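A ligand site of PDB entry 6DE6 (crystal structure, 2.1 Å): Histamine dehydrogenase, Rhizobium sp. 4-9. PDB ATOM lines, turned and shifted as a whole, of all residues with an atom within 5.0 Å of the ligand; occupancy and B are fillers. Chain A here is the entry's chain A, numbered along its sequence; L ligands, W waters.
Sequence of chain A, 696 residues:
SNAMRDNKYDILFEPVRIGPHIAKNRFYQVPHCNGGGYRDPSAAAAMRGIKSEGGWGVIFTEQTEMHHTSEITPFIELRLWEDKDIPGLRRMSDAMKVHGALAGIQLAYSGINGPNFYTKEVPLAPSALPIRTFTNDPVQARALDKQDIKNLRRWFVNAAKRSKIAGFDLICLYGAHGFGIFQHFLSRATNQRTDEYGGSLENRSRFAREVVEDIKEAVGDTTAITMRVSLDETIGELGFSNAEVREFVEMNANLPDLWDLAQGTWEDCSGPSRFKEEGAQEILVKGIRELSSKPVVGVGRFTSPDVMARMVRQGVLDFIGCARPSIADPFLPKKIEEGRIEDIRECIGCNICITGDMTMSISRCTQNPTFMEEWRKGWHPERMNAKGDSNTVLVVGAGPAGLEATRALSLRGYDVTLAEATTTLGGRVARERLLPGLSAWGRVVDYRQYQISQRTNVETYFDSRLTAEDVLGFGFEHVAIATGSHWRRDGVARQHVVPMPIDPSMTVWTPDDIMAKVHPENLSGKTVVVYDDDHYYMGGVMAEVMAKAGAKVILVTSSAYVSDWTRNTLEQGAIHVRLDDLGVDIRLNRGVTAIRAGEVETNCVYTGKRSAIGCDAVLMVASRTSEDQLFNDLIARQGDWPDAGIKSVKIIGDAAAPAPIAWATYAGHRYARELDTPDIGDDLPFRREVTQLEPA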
ATOM      1  N   VAL A  30      -8.336  -7.785 -20.589  1.00  0.00           N
ATOM      2  CA  VAL A  30      -8.254  -9.129 -21.155  1.00  0.00           C
ATOM      3  C   VAL A  30      -9.664  -9.566 -21.536  1.00  0.00           C
ATOM      4  O   VAL A  30     -10.654  -8.980 -21.083  1.00  0.00           O
ATOM      5  CB  VAL A  30      -7.601 -10.108 -20.167  1.00  0.00           C
ATOM      6  CG1 VAL A  30      -6.124  -9.773 -19.946  1.00  0.00           C
ATOM      7  CG2 VAL A  30      -8.327 -10.113 -18.826  1.00  0.00           C
ATOM      8  N   PRO A  31      -9.800 -10.551 -22.397  1.00  0.00           N
ATOM      9  CA  PRO A  31     -11.135 -11.022 -22.767  1.00  0.00           C
ATOM     10  C   PRO A  31     -11.942 -11.441 -21.546  1.00  0.00           C
ATOM     11  O   PRO A  31     -11.448 -12.165 -20.674  1.00  0.00           O
ATOM     12  CB  PRO A  31     -10.843 -12.208 -23.708  1.00  0.00           C
ATOM     13  CG  PRO A  31      -9.443 -11.983 -24.174  1.00  0.00           C
ATOM     14  CD  PRO A  31      -8.717 -11.306 -23.067  1.00  0.00           C
ATOM     15  N   HIS A  32     -13.182 -10.983 -21.463  1.00  0.00           N
ATOM     16  CA  HIS A  32     -14.049 -11.452 -20.409  1.00  0.00           C
ATOM     17  C   HIS A  32     -15.512 -11.413 -20.853  1.00  0.00           C
ATOM     18  O   HIS A  32     -15.923 -10.554 -21.643  1.00  0.00           O
ATOM     19  CB  HIS A  32     -13.805 -10.674 -19.087  1.00  0.00           C
ATOM     20  CG  HIS A  32     -14.370  -9.278 -19.033  1.00  0.00           C
ATOM     21  ND1 HIS A  32     -15.726  -9.007 -18.963  1.00  0.00           N
ATOM     22  CD2 HIS A  32     -13.755  -8.079 -18.903  1.00  0.00           C
ATOM     23  CE1 HIS A  32     -15.912  -7.707 -18.866  1.00  0.00           C
ATOM     24  NE2 HIS A  32     -14.743  -7.112 -18.808  1.00  0.00           N
ATOM     25  N   CYS A  33     -16.277 -12.357 -20.315  1.00  0.00           N
ATOM     26  CA  CYS A  33     -17.679 -12.575 -20.607  1.00  0.00           C
ATOM     27  C   CYS A  33     -18.511 -11.578 -19.819  1.00  0.00           C
ATOM     28  O   CYS A  33     -18.010 -10.865 -18.946  1.00  0.00           O
ATOM     29  CB  CYS A  33     -18.084 -14.008 -20.253  1.00  0.00           C
ATOM     30  SG  CYS A  33     -17.744 -14.543 -18.563  1.00  0.00           S
ATOM     31  N   ASN A  34     -19.803 -11.563 -20.094  1.00  0.00           N
ATOM     32  CA  ASN A  34     -20.685 -10.569 -19.489  1.00  0.00           C
ATOM     33  C   ASN A  34     -22.141 -11.023 -19.409  1.00  0.00           C
ATOM     34  O   ASN A  34     -23.001 -10.209 -19.035  1.00  0.00           O
ATOM     35  CB  ASN A  34     -20.599  -9.257 -20.287  1.00  0.00           C
ATOM     36  CG  ASN A  34     -20.838  -9.461 -21.770  1.00  0.00           C
ATOM     37  OD1 ASN A  34     -21.927  -9.907 -22.191  1.00  0.00           O
ATOM     38  ND2 ASN A  34     -19.820  -9.178 -22.581  1.00  0.00           N
ATOM     39  N   GLU A  62     -15.336 -10.960 -25.127  1.00  0.00           N
ATOM     40  CA  GLU A  62     -15.331 -12.333 -24.615  1.00  0.00           C
ATOM     41  C   GLU A  62     -14.977 -13.313 -25.738  1.00  0.00           C
ATOM     42  O   GLU A  62     -14.880 -12.953 -26.923  1.00  0.00           O
ATOM     43  CB  GLU A  62     -16.707 -12.680 -24.038  1.00  0.00           C
ATOM     44  CG  GLU A  62     -17.876 -12.532 -25.037  1.00  0.00           C
ATOM     45  CD  GLU A  62     -18.560 -11.151 -25.035  1.00  0.00           C
ATOM     46  OE1 GLU A  62     -17.866 -10.107 -25.198  1.00  0.00           O
ATOM     47  OE2 GLU A  62     -19.797 -11.091 -24.850  1.00  0.00           O
ATOM     48  N   GLN A  63     -14.809 -14.587 -25.379  1.00  0.00           N
ATOM     49  CA  GLN A  63     -14.516 -15.567 -26.423  1.00  0.00           C
ATOM     50  C   GLN A  63     -15.600 -15.532 -27.492  1.00  0.00           C
ATOM     51  O   GLN A  63     -16.785 -15.293 -27.204  1.00  0.00           O
ATOM     52  CB  GLN A  63     -14.376 -16.988 -25.854  1.00  0.00           C
ATOM     53  CG  GLN A  63     -15.654 -17.576 -25.300  1.00  0.00           C
ATOM     54  CD  GLN A  63     -15.587 -19.062 -25.111  1.00  0.00           C
ATOM     55  OE1 GLN A  63     -15.528 -19.831 -26.075  1.00  0.00           O
ATOM     56  NE2 GLN A  63     -15.625 -19.489 -23.873  1.00  0.00           N
ATOM     57  N   GLU A  77     -21.806 -16.632 -25.276  1.00  0.00           N
ATOM     58  CA  GLU A  77     -20.670 -15.762 -25.538  1.00  0.00           C
ATOM     59  C   GLU A  77     -20.916 -15.062 -26.867  1.00  0.00           C
ATOM     60  O   GLU A  77     -22.045 -14.597 -27.095  1.00  0.00           O
ATOM     61  CB  GLU A  77     -19.390 -16.573 -25.472  1.00  0.00           C
ATOM     62  CG  GLU A  77     -19.248 -17.501 -24.308  1.00  0.00           C
ATOM     63  CD  GLU A  77     -19.460 -16.837 -22.948  1.00  0.00           C
ATOM     64  OE1 GLU A  77     -19.239 -15.611 -22.799  1.00  0.00           O
ATOM     65  OE2 GLU A  77     -19.807 -17.568 -22.029  1.00  0.00           O
ATOM     66  N   GLN A 106     -11.430 -12.008 -29.303  1.00  0.00           N
ATOM     67  CA  GLN A 106     -10.907 -13.319 -28.955  1.00  0.00           C
ATOM     68  C   GLN A 106     -11.671 -14.373 -29.731  1.00  0.00           C
ATOM     69  O   GLN A 106     -12.900 -14.398 -29.723  1.00  0.00           O
ATOM     70  CB  GLN A 106     -11.006 -13.580 -27.455  1.00  0.00           C
ATOM     71  CG  GLN A 106     -10.371 -14.908 -26.991  1.00  0.00           C
ATOM     72  CD  GLN A 106     -10.628 -15.164 -25.505  1.00  0.00           C
ATOM     73  OE1 GLN A 106     -11.788 -15.191 -25.075  1.00  0.00           O
ATOM     74  NE2 GLN A 106      -9.566 -15.330 -24.730  1.00  0.00           N
ATOM     75  N   TYR A 174      -7.589 -18.135 -28.319  1.00  0.00           N
ATOM     76  CA  TYR A 174      -7.931 -18.551 -26.969  1.00  0.00           C
ATOM     77  C   TYR A 174      -7.378 -19.929 -26.643  1.00  0.00           C
ATOM     78  O   TYR A 174      -7.786 -20.931 -27.257  1.00  0.00           O
ATOM     79  CB  TYR A 174      -9.450 -18.583 -26.804  1.00  0.00           C
ATOM     80  CG  TYR A 174      -9.936 -18.747 -25.368  1.00  0.00           C
ATOM     81  CD1 TYR A 174      -9.106 -18.504 -24.286  1.00  0.00           C
ATOM     82  CD2 TYR A 174     -11.225 -19.188 -25.119  1.00  0.00           C
ATOM     83  CE1 TYR A 174      -9.550 -18.662 -22.994  1.00  0.00           C
ATOM     84  CE2 TYR A 174     -11.687 -19.352 -23.820  1.00  0.00           C
ATOM     85  CZ  TYR A 174     -10.853 -19.097 -22.773  1.00  0.00           C
ATOM     86  OH  TYR A 174     -11.333 -19.251 -21.509  1.00  0.00           O
ATOM     87  N   HIS A 177      -7.286 -21.562 -19.536  1.00  0.00           N
ATOM     88  CA  HIS A 177      -8.324 -22.172 -18.697  1.00  0.00           C
ATOM     89  C   HIS A 177      -8.554 -23.620 -19.056  1.00  0.00           C
ATOM     90  O   HIS A 177      -9.634 -24.159 -18.843  1.00  0.00           O
ATOM     91  CB  HIS A 177      -9.620 -21.371 -18.785  1.00  0.00           C
ATOM     92  CG  HIS A 177      -9.422 -19.916 -18.495  1.00  0.00           C
ATOM     93  ND1 HIS A 177      -9.783 -18.912 -19.363  1.00  0.00           N
ATOM     94  CD2 HIS A 177      -8.817 -19.310 -17.446  1.00  0.00           C
ATOM     95  CE1 HIS A 177      -9.436 -17.748 -18.852  1.00  0.00           C
ATOM     96  NE2 HIS A 177      -8.861 -17.953 -17.675  1.00  0.00           N
ATOM     97  N   ARG A 228      -3.464 -16.520 -25.984  1.00  0.00           N
ATOM     98  CA  ARG A 228      -3.742 -16.606 -24.555  1.00  0.00           C
ATOM     99  C   ARG A 228      -3.490 -18.047 -24.152  1.00  0.00           C
ATOM    100  O   ARG A 228      -4.113 -18.971 -24.685  1.00  0.00           O
ATOM    101  CB  ARG A 228      -5.162 -16.152 -24.212  1.00  0.00           C
ATOM    102  CG  ARG A 228      -5.367 -15.913 -22.712  1.00  0.00           C
ATOM    103  CD  ARG A 228      -6.500 -14.933 -22.395  1.00  0.00           C
ATOM    104  NE  ARG A 228      -6.262 -14.260 -21.134  1.00  0.00           N
ATOM    105  CZ  ARG A 228      -7.120 -14.152 -20.121  1.00  0.00           C
ATOM    106  NH1 ARG A 228      -8.338 -14.669 -20.193  1.00  0.00           N
ATOM    107  NH2 ARG A 228      -6.741 -13.472 -19.041  1.00  0.00           N
ATOM    108  N   ALA A 262      -2.559 -16.695 -18.718  1.00  0.00           N
ATOM    109  CA  ALA A 262      -3.634 -16.922 -17.768  1.00  0.00           C
ATOM    110  C   ALA A 262      -3.528 -18.325 -17.179  1.00  0.00           C
ATOM    111  O   ALA A 262      -2.789 -19.173 -17.682  1.00  0.00           O
ATOM    112  CB  ALA A 262      -5.001 -16.697 -18.416  1.00  0.00           C
ATOM    113  N   TRP A 266     -10.465 -21.921 -15.140  1.00  0.00           N
ATOM    114  CA  TRP A 266     -11.156 -20.690 -14.796  1.00  0.00           C
ATOM    115  C   TRP A 266     -11.244 -20.505 -13.285  1.00  0.00           C
ATOM    116  O   TRP A 266     -11.039 -19.404 -12.760  1.00  0.00           O
ATOM    117  CB  TRP A 266     -12.552 -20.708 -15.412  1.00  0.00           C
ATOM    118  CG  TRP A 266     -13.188 -19.387 -15.492  1.00  0.00           C
ATOM    119  CD1 TRP A 266     -12.645 -18.176 -15.160  1.00  0.00           C
ATOM    120  CD2 TRP A 266     -14.509 -19.118 -15.929  1.00  0.00           C
ATOM    121  NE1 TRP A 266     -13.552 -17.176 -15.367  1.00  0.00           N
ATOM    122  CE2 TRP A 266     -14.706 -17.723 -15.847  1.00  0.00           C
ATOM    123  CE3 TRP A 266     -15.555 -19.927 -16.399  1.00  0.00           C
ATOM    124  CZ2 TRP A 266     -15.906 -17.120 -16.199  1.00  0.00           C
ATOM    125  CZ3 TRP A 266     -16.756 -19.316 -16.745  1.00  0.00           C
ATOM    126  CH2 TRP A 266     -16.920 -17.928 -16.648  1.00  0.00           C
ATOM    127  N   CYS A 269      -8.007 -19.102 -12.231  1.00  0.00           N
ATOM    128  CA  CYS A 269      -7.665 -17.809 -12.816  1.00  0.00           C
ATOM    129  C   CYS A 269      -8.451 -16.671 -12.174  1.00  0.00           C
ATOM    130  O   CYS A 269      -7.869 -15.682 -11.707  1.00  0.00           O
ATOM    131  CB  CYS A 269      -7.906 -17.861 -14.327  1.00  0.00           C
ATOM    132  SG  CYS A 269      -7.040 -16.590 -15.254  1.00  0.00           S
ATOM    133  N   SER A 270      -9.788 -16.795 -12.129  1.00  0.00           N
ATOM    134  CA  SER A 270     -10.644 -15.803 -11.463  1.00  0.00           C
ATOM    135  C   SER A 270     -10.666 -16.115  -9.963  1.00  0.00           C
ATOM    136  O   SER A 270     -11.679 -16.532  -9.384  1.00  0.00           O
ATOM    137  CB  SER A 270     -12.042 -15.809 -12.044  1.00  0.00           C
ATOM    138  OG  SER A 270     -12.063 -15.438 -13.425  1.00  0.00           O
ATOM    139  N   VAL A 299      -2.551 -11.408 -15.415  1.00  0.00           N
ATOM    140  CA  VAL A 299      -3.619 -11.004 -14.514  1.00  0.00           C
ATOM    141  C   VAL A 299      -3.266 -11.366 -13.074  1.00  0.00           C
ATOM    142  O   VAL A 299      -2.324 -12.119 -12.794  1.00  0.00           O
ATOM    143  CB  VAL A 299      -4.979 -11.617 -14.914  1.00  0.00           C
ATOM    144  CG1 VAL A 299      -5.425 -11.065 -16.257  1.00  0.00           C
ATOM    145  CG2 VAL A 299      -4.880 -13.160 -14.955  1.00  0.00           C
ATOM    146  N   GLY A 300      -4.040 -10.809 -12.150  1.00  0.00           N
ATOM    147  CA  GLY A 300      -3.819 -11.029 -10.726  1.00  0.00           C
ATOM    148  C   GLY A 300      -4.793 -10.322  -9.808  1.00  0.00           C
ATOM    149  O   GLY A 300      -4.433  -9.935  -8.694  1.00  0.00           O
ATOM    150  N   ARG A 301      -6.043 -10.173 -10.270  1.00  0.00           N
ATOM    151  CA  ARG A 301      -7.038  -9.309  -9.618  1.00  0.00           C
ATOM    152  C   ARG A 301      -6.410  -7.983  -9.191  1.00  0.00           C
ATOM    153  O   ARG A 301      -6.496  -7.537  -8.044  1.00  0.00           O
ATOM    154  CB  ARG A 301      -7.696 -10.026  -8.434  1.00  0.00           C
ATOM    155  CG  ARG A 301      -9.064  -9.479  -8.041  1.00  0.00           C
ATOM    156  CD  ARG A 301      -9.768 -10.375  -7.030  1.00  0.00           C
ATOM    157  NE  ARG A 301      -9.135 -10.266  -5.714  1.00  0.00           N
ATOM    158  CZ  ARG A 301      -8.477 -11.230  -5.068  1.00  0.00           C
ATOM    159  NH1 ARG A 301      -8.358 -12.471  -5.582  1.00  0.00           N
ATOM    160  NH2 ARG A 301      -7.954 -10.947  -3.883  1.00  0.00           N
ATOM    161  N   PHE A 302      -5.743  -7.339 -10.143  1.00  0.00           N
ATOM    162  CA  PHE A 302      -4.969  -6.134  -9.871  1.00  0.00           C
ATOM    163  C   PHE A 302      -5.901  -4.961  -9.553  1.00  0.00           C
ATOM    164  O   PHE A 302      -6.523  -4.387 -10.460  1.00  0.00           O
ATOM    165  CB  PHE A 302      -4.076  -5.812 -11.061  1.00  0.00           C
ATOM    166  CG  PHE A 302      -2.998  -6.838 -11.303  1.00  0.00           C
ATOM    167  CD1 PHE A 302      -2.228  -7.307 -10.240  1.00  0.00           C
ATOM    168  CD2 PHE A 302      -2.760  -7.340 -12.555  1.00  0.00           C
ATOM    169  CE1 PHE A 302      -1.227  -8.244 -10.446  1.00  0.00           C
ATOM    170  CE2 PHE A 302      -1.766  -8.298 -12.768  1.00  0.00           C
ATOM    171  CZ  PHE A 302      -1.008  -8.741 -11.710  1.00  0.00           C
ATOM    172  N   GLY A 321      -2.955  -6.699 -17.023  1.00  0.00           N
ATOM    173  CA  GLY A 321      -4.201  -7.276 -17.475  1.00  0.00           C
ATOM    174  C   GLY A 321      -5.241  -7.261 -16.374  1.00  0.00           C
ATOM    175  O   GLY A 321      -4.966  -7.687 -15.244  1.00  0.00           O
ATOM    176  N   CYS A 322      -6.458  -6.837 -16.717  1.00  0.00           N
ATOM    177  CA  CYS A 322      -7.546  -6.809 -15.750  1.00  0.00           C
ATOM    178  C   CYS A 322      -8.811  -7.300 -16.419  1.00  0.00           C
ATOM    179  O   CYS A 322      -9.116  -6.921 -17.557  1.00  0.00           O
ATOM    180  CB  CYS A 322      -7.790  -5.411 -15.219  1.00  0.00           C
ATOM    181  SG  CYS A 322      -6.421  -4.742 -14.349  1.00  0.00           S
ATOM    182  N   ALA A 323      -9.522  -8.172 -15.710  1.00  0.00           N
ATOM    183  CA  ALA A 323     -10.904  -8.456 -16.043  1.00  0.00           C
ATOM    184  C   ALA A 323     -11.781  -7.889 -14.939  1.00  0.00           C
ATOM    185  O   ALA A 323     -12.338  -6.799 -15.077  1.00  0.00           O
ATOM    186  CB  ALA A 323     -11.104  -9.954 -16.237  1.00  0.00           C
ATOM    187  N   ARG A 324     -11.861  -8.578 -13.805  1.00  0.00           N
ATOM    188  CA  ARG A 324     -12.769  -8.135 -12.756  1.00  0.00           C
ATOM    189  C   ARG A 324     -12.469  -6.739 -12.220  1.00  0.00           C
ATOM    190  O   ARG A 324     -13.429  -5.985 -11.953  1.00  0.00           O
ATOM    191  CB  ARG A 324     -12.761  -9.158 -11.617  1.00  0.00           C
ATOM    192  CG  ARG A 324     -13.458 -10.479 -12.010  1.00  0.00           C
ATOM    193  CD  ARG A 324     -13.197 -11.574 -11.026  1.00  0.00           C
ATOM    194  NE  ARG A 324     -11.774 -11.820 -10.909  1.00  0.00           N
ATOM    195  CZ  ARG A 324     -11.203 -12.489  -9.907  1.00  0.00           C
ATOM    196  NH1 ARG A 324     -11.957 -12.996  -8.921  1.00  0.00           N
ATOM    197  NH2 ARG A 324      -9.900 -12.614  -9.880  1.00  0.00           N
ATOM    198  N   PRO A 325     -11.213  -6.308 -12.051  1.00  0.00           N
ATOM    199  CA  PRO A 325     -10.974  -4.914 -11.610  1.00  0.00           C
ATOM    200  C   PRO A 325     -11.527  -3.870 -12.570  1.00  0.00           C
ATOM    201  O   PRO A 325     -11.879  -2.761 -12.133  1.00  0.00           O
ATOM    202  CB  PRO A 325      -9.452  -4.819 -11.511  1.00  0.00           C
ATOM    203  CG  PRO A 325      -8.989  -6.275 -11.281  1.00  0.00           C
ATOM    204  CD  PRO A 325      -9.977  -7.119 -12.064  1.00  0.00           C
ATOM    205  N   ILE A 327     -14.285  -4.407 -14.399  1.00  0.00           N
ATOM    206  CA  ILE A 327     -15.725  -4.462 -14.205  1.00  0.00           C
ATOM    207  C   ILE A 327     -16.141  -3.638 -12.990  1.00  0.00           C
ATOM    208  O   ILE A 327     -17.053  -2.815 -13.046  1.00  0.00           O
ATOM    209  CB  ILE A 327     -16.181  -5.934 -14.070  1.00  0.00           C
ATOM    210  CG1 ILE A 327     -15.935  -6.674 -15.366  1.00  0.00           C
ATOM    211  CG2 ILE A 327     -17.663  -6.013 -13.636  1.00  0.00           C
ATOM    212  CD1 ILE A 327     -16.026  -8.192 -15.228  1.00  0.00           C
ATOM    213  N   CYS A 353     -20.021 -11.587 -10.785  1.00  0.00           N
ATOM    214  CA  CYS A 353     -20.005 -11.357 -12.237  1.00  0.00           C
ATOM    215  C   CYS A 353     -20.010 -12.655 -13.027  1.00  0.00           C
ATOM    216  O   CYS A 353     -20.653 -12.749 -14.099  1.00  0.00           O
ATOM    217  CB  CYS A 353     -18.769 -10.518 -12.597  1.00  0.00           C
ATOM    218  SG  CYS A 353     -17.228 -11.058 -11.799  1.00  0.00           S
ATOM    219  N   ILE A 354     -19.295 -13.671 -12.544  1.00  0.00           N
ATOM    220  CA  ILE A 354     -19.239 -14.971 -13.214  1.00  0.00           C
ATOM    221  C   ILE A 354     -20.584 -15.660 -13.146  1.00  0.00           C
ATOM    222  O   ILE A 354     -20.940 -16.429 -14.055  1.00  0.00           O
ATOM    223  CB  ILE A 354     -18.109 -15.809 -12.584  1.00  0.00           C
ATOM    224  CG1 ILE A 354     -16.772 -15.126 -12.876  1.00  0.00           C
ATOM    225  CG2 ILE A 354     -18.093 -17.259 -13.131  1.00  0.00           C
ATOM    226  CD1 ILE A 354     -15.602 -15.795 -12.237  1.00  0.00           C
ATOM    227  N   ASP A 357     -22.585 -15.241 -16.279  1.00  0.00           N
ATOM    228  CA  ASP A 357     -22.205 -16.141 -17.371  1.00  0.00           C
ATOM    229  C   ASP A 357     -22.718 -17.552 -17.122  1.00  0.00           C
ATOM    230  O   ASP A 357     -23.248 -18.198 -18.028  1.00  0.00           O
ATOM    231  CB  ASP A 357     -20.688 -16.129 -17.507  1.00  0.00           C
ATOM    232  CG  ASP A 357     -20.176 -17.036 -18.622  1.00  0.00           C
ATOM    233  OD1 ASP A 357     -20.187 -16.589 -19.790  1.00  0.00           O
ATOM    234  OD2 ASP A 357     -19.746 -18.183 -18.315  1.00  0.00           O
ATOM    235  N   SER A 363     -24.438 -10.110 -16.632  1.00  0.00           N
ATOM    236  CA  SER A 363     -23.692 -10.116 -15.378  1.00  0.00           C
ATOM    237  C   SER A 363     -23.963  -8.848 -14.590  1.00  0.00           C
ATOM    238  O   SER A 363     -24.171  -7.762 -15.144  1.00  0.00           O
ATOM    239  CB  SER A 363     -22.181 -10.204 -15.652  1.00  0.00           C
ATOM    240  OG  SER A 363     -21.854 -11.387 -16.360  1.00  0.00           O
HETATM  241  N1  LIG L   1     -11.138 -15.295 -20.159  1.00  0.00           N
HETATM  242  C1  LIG L   1     -11.025 -15.519 -21.590  1.00  0.00           C
HETATM  243  O1  LIG L   1      -9.950 -15.702 -22.066  1.00  0.00           O
HETATM  244  N2  LIG L   1     -12.259 -15.548 -22.412  1.00  0.00           N
HETATM  245  C2  LIG L   1     -13.561 -15.311 -21.822  1.00  0.00           C
HETATM  246  O2  LIG L   1     -14.548 -15.328 -22.477  1.00  0.00           O
HETATM  247  C3  LIG L   1     -13.641 -15.065 -20.346  1.00  0.00           C
HETATM  248  N3  LIG L   1     -14.921 -14.830 -19.731  1.00  0.00           N
HETATM  249  C4  LIG L   1     -14.996 -14.543 -18.261  1.00  0.00           C
HETATM  250  C5  LIG L   1     -16.196 -13.982 -17.754  1.00  0.00           C
HETATM  251  C6  LIG L   1     -16.136 -13.228 -16.569  1.00  0.00           C
HETATM  252  C7  LIG L   1     -17.517 -12.820 -16.064  1.00  0.00           C
HETATM  253  C8  LIG L   1     -14.923 -13.147 -15.861  1.00  0.00           C
HETATM  254  C9  LIG L   1     -14.873 -12.406 -14.517  1.00  0.00           C
HETATM  255  C10 LIG L   1     -13.781 -13.762 -16.337  1.00  0.00           C
HETATM  256  C11 LIG L   1     -13.805 -14.514 -17.517  1.00  0.00           C
HETATM  257  N4  LIG L   1     -12.491 -14.776 -18.158  1.00  0.00           N
HETATM  258  C12 LIG L   1     -12.432 -15.046 -19.567  1.00  0.00           C
HETATM  259  C13 LIG L   1     -11.241 -14.797 -17.402  1.00  0.00           C
HETATM  260  C14 LIG L   1     -10.624 -13.405 -17.303  1.00  0.00           C
HETATM  261  O3  LIG L   1     -10.190 -13.022 -18.572  1.00  0.00           O
HETATM  262  C15 LIG L   1      -9.415 -13.363 -16.362  1.00  0.00           C
HETATM  263  O4  LIG L   1      -8.425 -14.244 -16.848  1.00  0.00           O
HETATM  264  C16 LIG L   1      -9.791 -13.765 -14.915  1.00  0.00           C
HETATM  265  O5  LIG L   1     -11.002 -13.182 -14.441  1.00  0.00           O
HETATM  266  C17 LIG L   1      -8.622 -13.343 -13.985  1.00  0.00           C
HETATM  267  O6  LIG L   1      -8.238 -12.000 -14.192  1.00  0.00           O
HETATM  268  P1  LIG L   1      -8.748 -10.843 -13.140  1.00  0.00           P
HETATM  269  O7  LIG L   1     -10.269 -10.877 -13.150  1.00  0.00           O
HETATM  270  O8  LIG L   1      -8.172 -11.217 -11.787  1.00  0.00           O
HETATM  271  O9  LIG L   1      -8.182  -9.524 -13.548  1.00  0.00           O
HETATM  272  O   HOH W   1      -5.887  -8.513 -12.951  1.00  0.00           O
HETATM  273  O   HOH W   2     -16.215 -17.412 -21.565  1.00  0.00           O
HETATM  274  O   HOH W   3      -6.515 -13.233 -11.375  1.00  0.00           O
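N of Cys 33 lies within hydrogen-bond range of N3 of the ligand, 2.9 Å away. SG of Cys 33 is bonded to C5 of the ligand. An oxygen (O3) of the ligand is in hydrogen-bond range of the backbone carbonyl oxygen of Pro 31, 2.6 Å away. The guanidinium group of Arg 228 lies within hydrogen-bond range of an oxygen (O1) of the ligand (2.7 Å). OG of Ser 270 lies within hydrogen-bond range of O5 of the ligand (2.7 Å). The side-chain amide nitrogen (NE2) of Gln 106 lies within hydrogen-bond range of an oxygen (O1) of the ligand, at 2.7 Å. The backbone NH of Arg 301 is in hydrogen-bond range of an oxygen (O8) of the ligand, 2.8 Å away. N of Arg 324 is in hydrogen-bond range of O7 of the ligand (2.9 Å). NE of Arg 324 is in salt-bridge range of O7 of the ligand (2.9 Å). The backbone NH (N) of Ala 323 is in hydrogen-bond range of an oxygen (O9) of the ligand (2.9 Å). O2 of the ligand lies within hydrogen-bond range of N of Gln 63 (3.0 Å). SG of Cys 269 lies within hydrogen-bond range of O4 of the ligand (3.2 Å).
The side-chain hydroxyl (OG) of Ser 270 sits at hydrogen-bond distance from the indole nitrogen (NE1) of Trp 266 (3.0 Å). N of Gln 63 sits close to OE1 of Gln 106 (3.1 Å). The side-chain hydroxyl (OH) of Tyr 174 sits at hydrogen-bond distance from a ring nitrogen (ND1) of His 177, 2.7 Å away. A ring nitrogen (NE2) of His 177 is in hydrogen-bond range of the side-chain sulfur (SG) of Cys 269, 3.3 Å away. The backbone NH (N) of Val 30 sits at hydrogen-bond distance from the backbone carbonyl oxygen (O) of Cys 322 (3.2 Å). The backbone carbonyl oxygen of Cys 353 is in hydrogen-bond range of the side-chain hydroxyl of Ser 363 (2.9 Å). ND2 of Asn 34 is in hydrogen-bond range of OE2 of Glu 62 (3.0 Å).
Val 30 touches the ligand. CA of His 32 touches N3 of the ligand, 3.6 Å away. Glu 62 touches the ligand. Tyr 174 touches the ligand. His 177 touches the ligand. Trp 266 touches the ligand. Val 299 touches the ligand (CB to O6, 3.4 Å). Cys 322 touches the ligand. CD of Pro 325 touches O9 of the ligand, at 3.3 Å. O of Cys 353 touches C7 of the ligand, 3.7 Å away. Ile 354 touches the ligand. 21 residues have an atom within 4 Å of the ligand: Val 30, Pro 31, His 32, Cys 33, Glu 62, Gln 63, Gln 106, Tyr 174, His 177, Arg 228, Trp 266, Cys 269, Ser 270, Val 299, Arg 301, Cys 322, Ala 323, Arg 324, Pro 325, Cys 353 and Ile 354.
Water W3 lies within hydrogen-bond range of O8 of the ligand (2.6 Å), O of Cys 269 (2.8 Å) and N of Arg 301 (3.3 Å). Water W2 lies within hydrogen-bond range of an oxygen (O2) of the ligand (2.8 Å) and the side-chain amide nitrogen of Gln 63 (3.2 Å).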
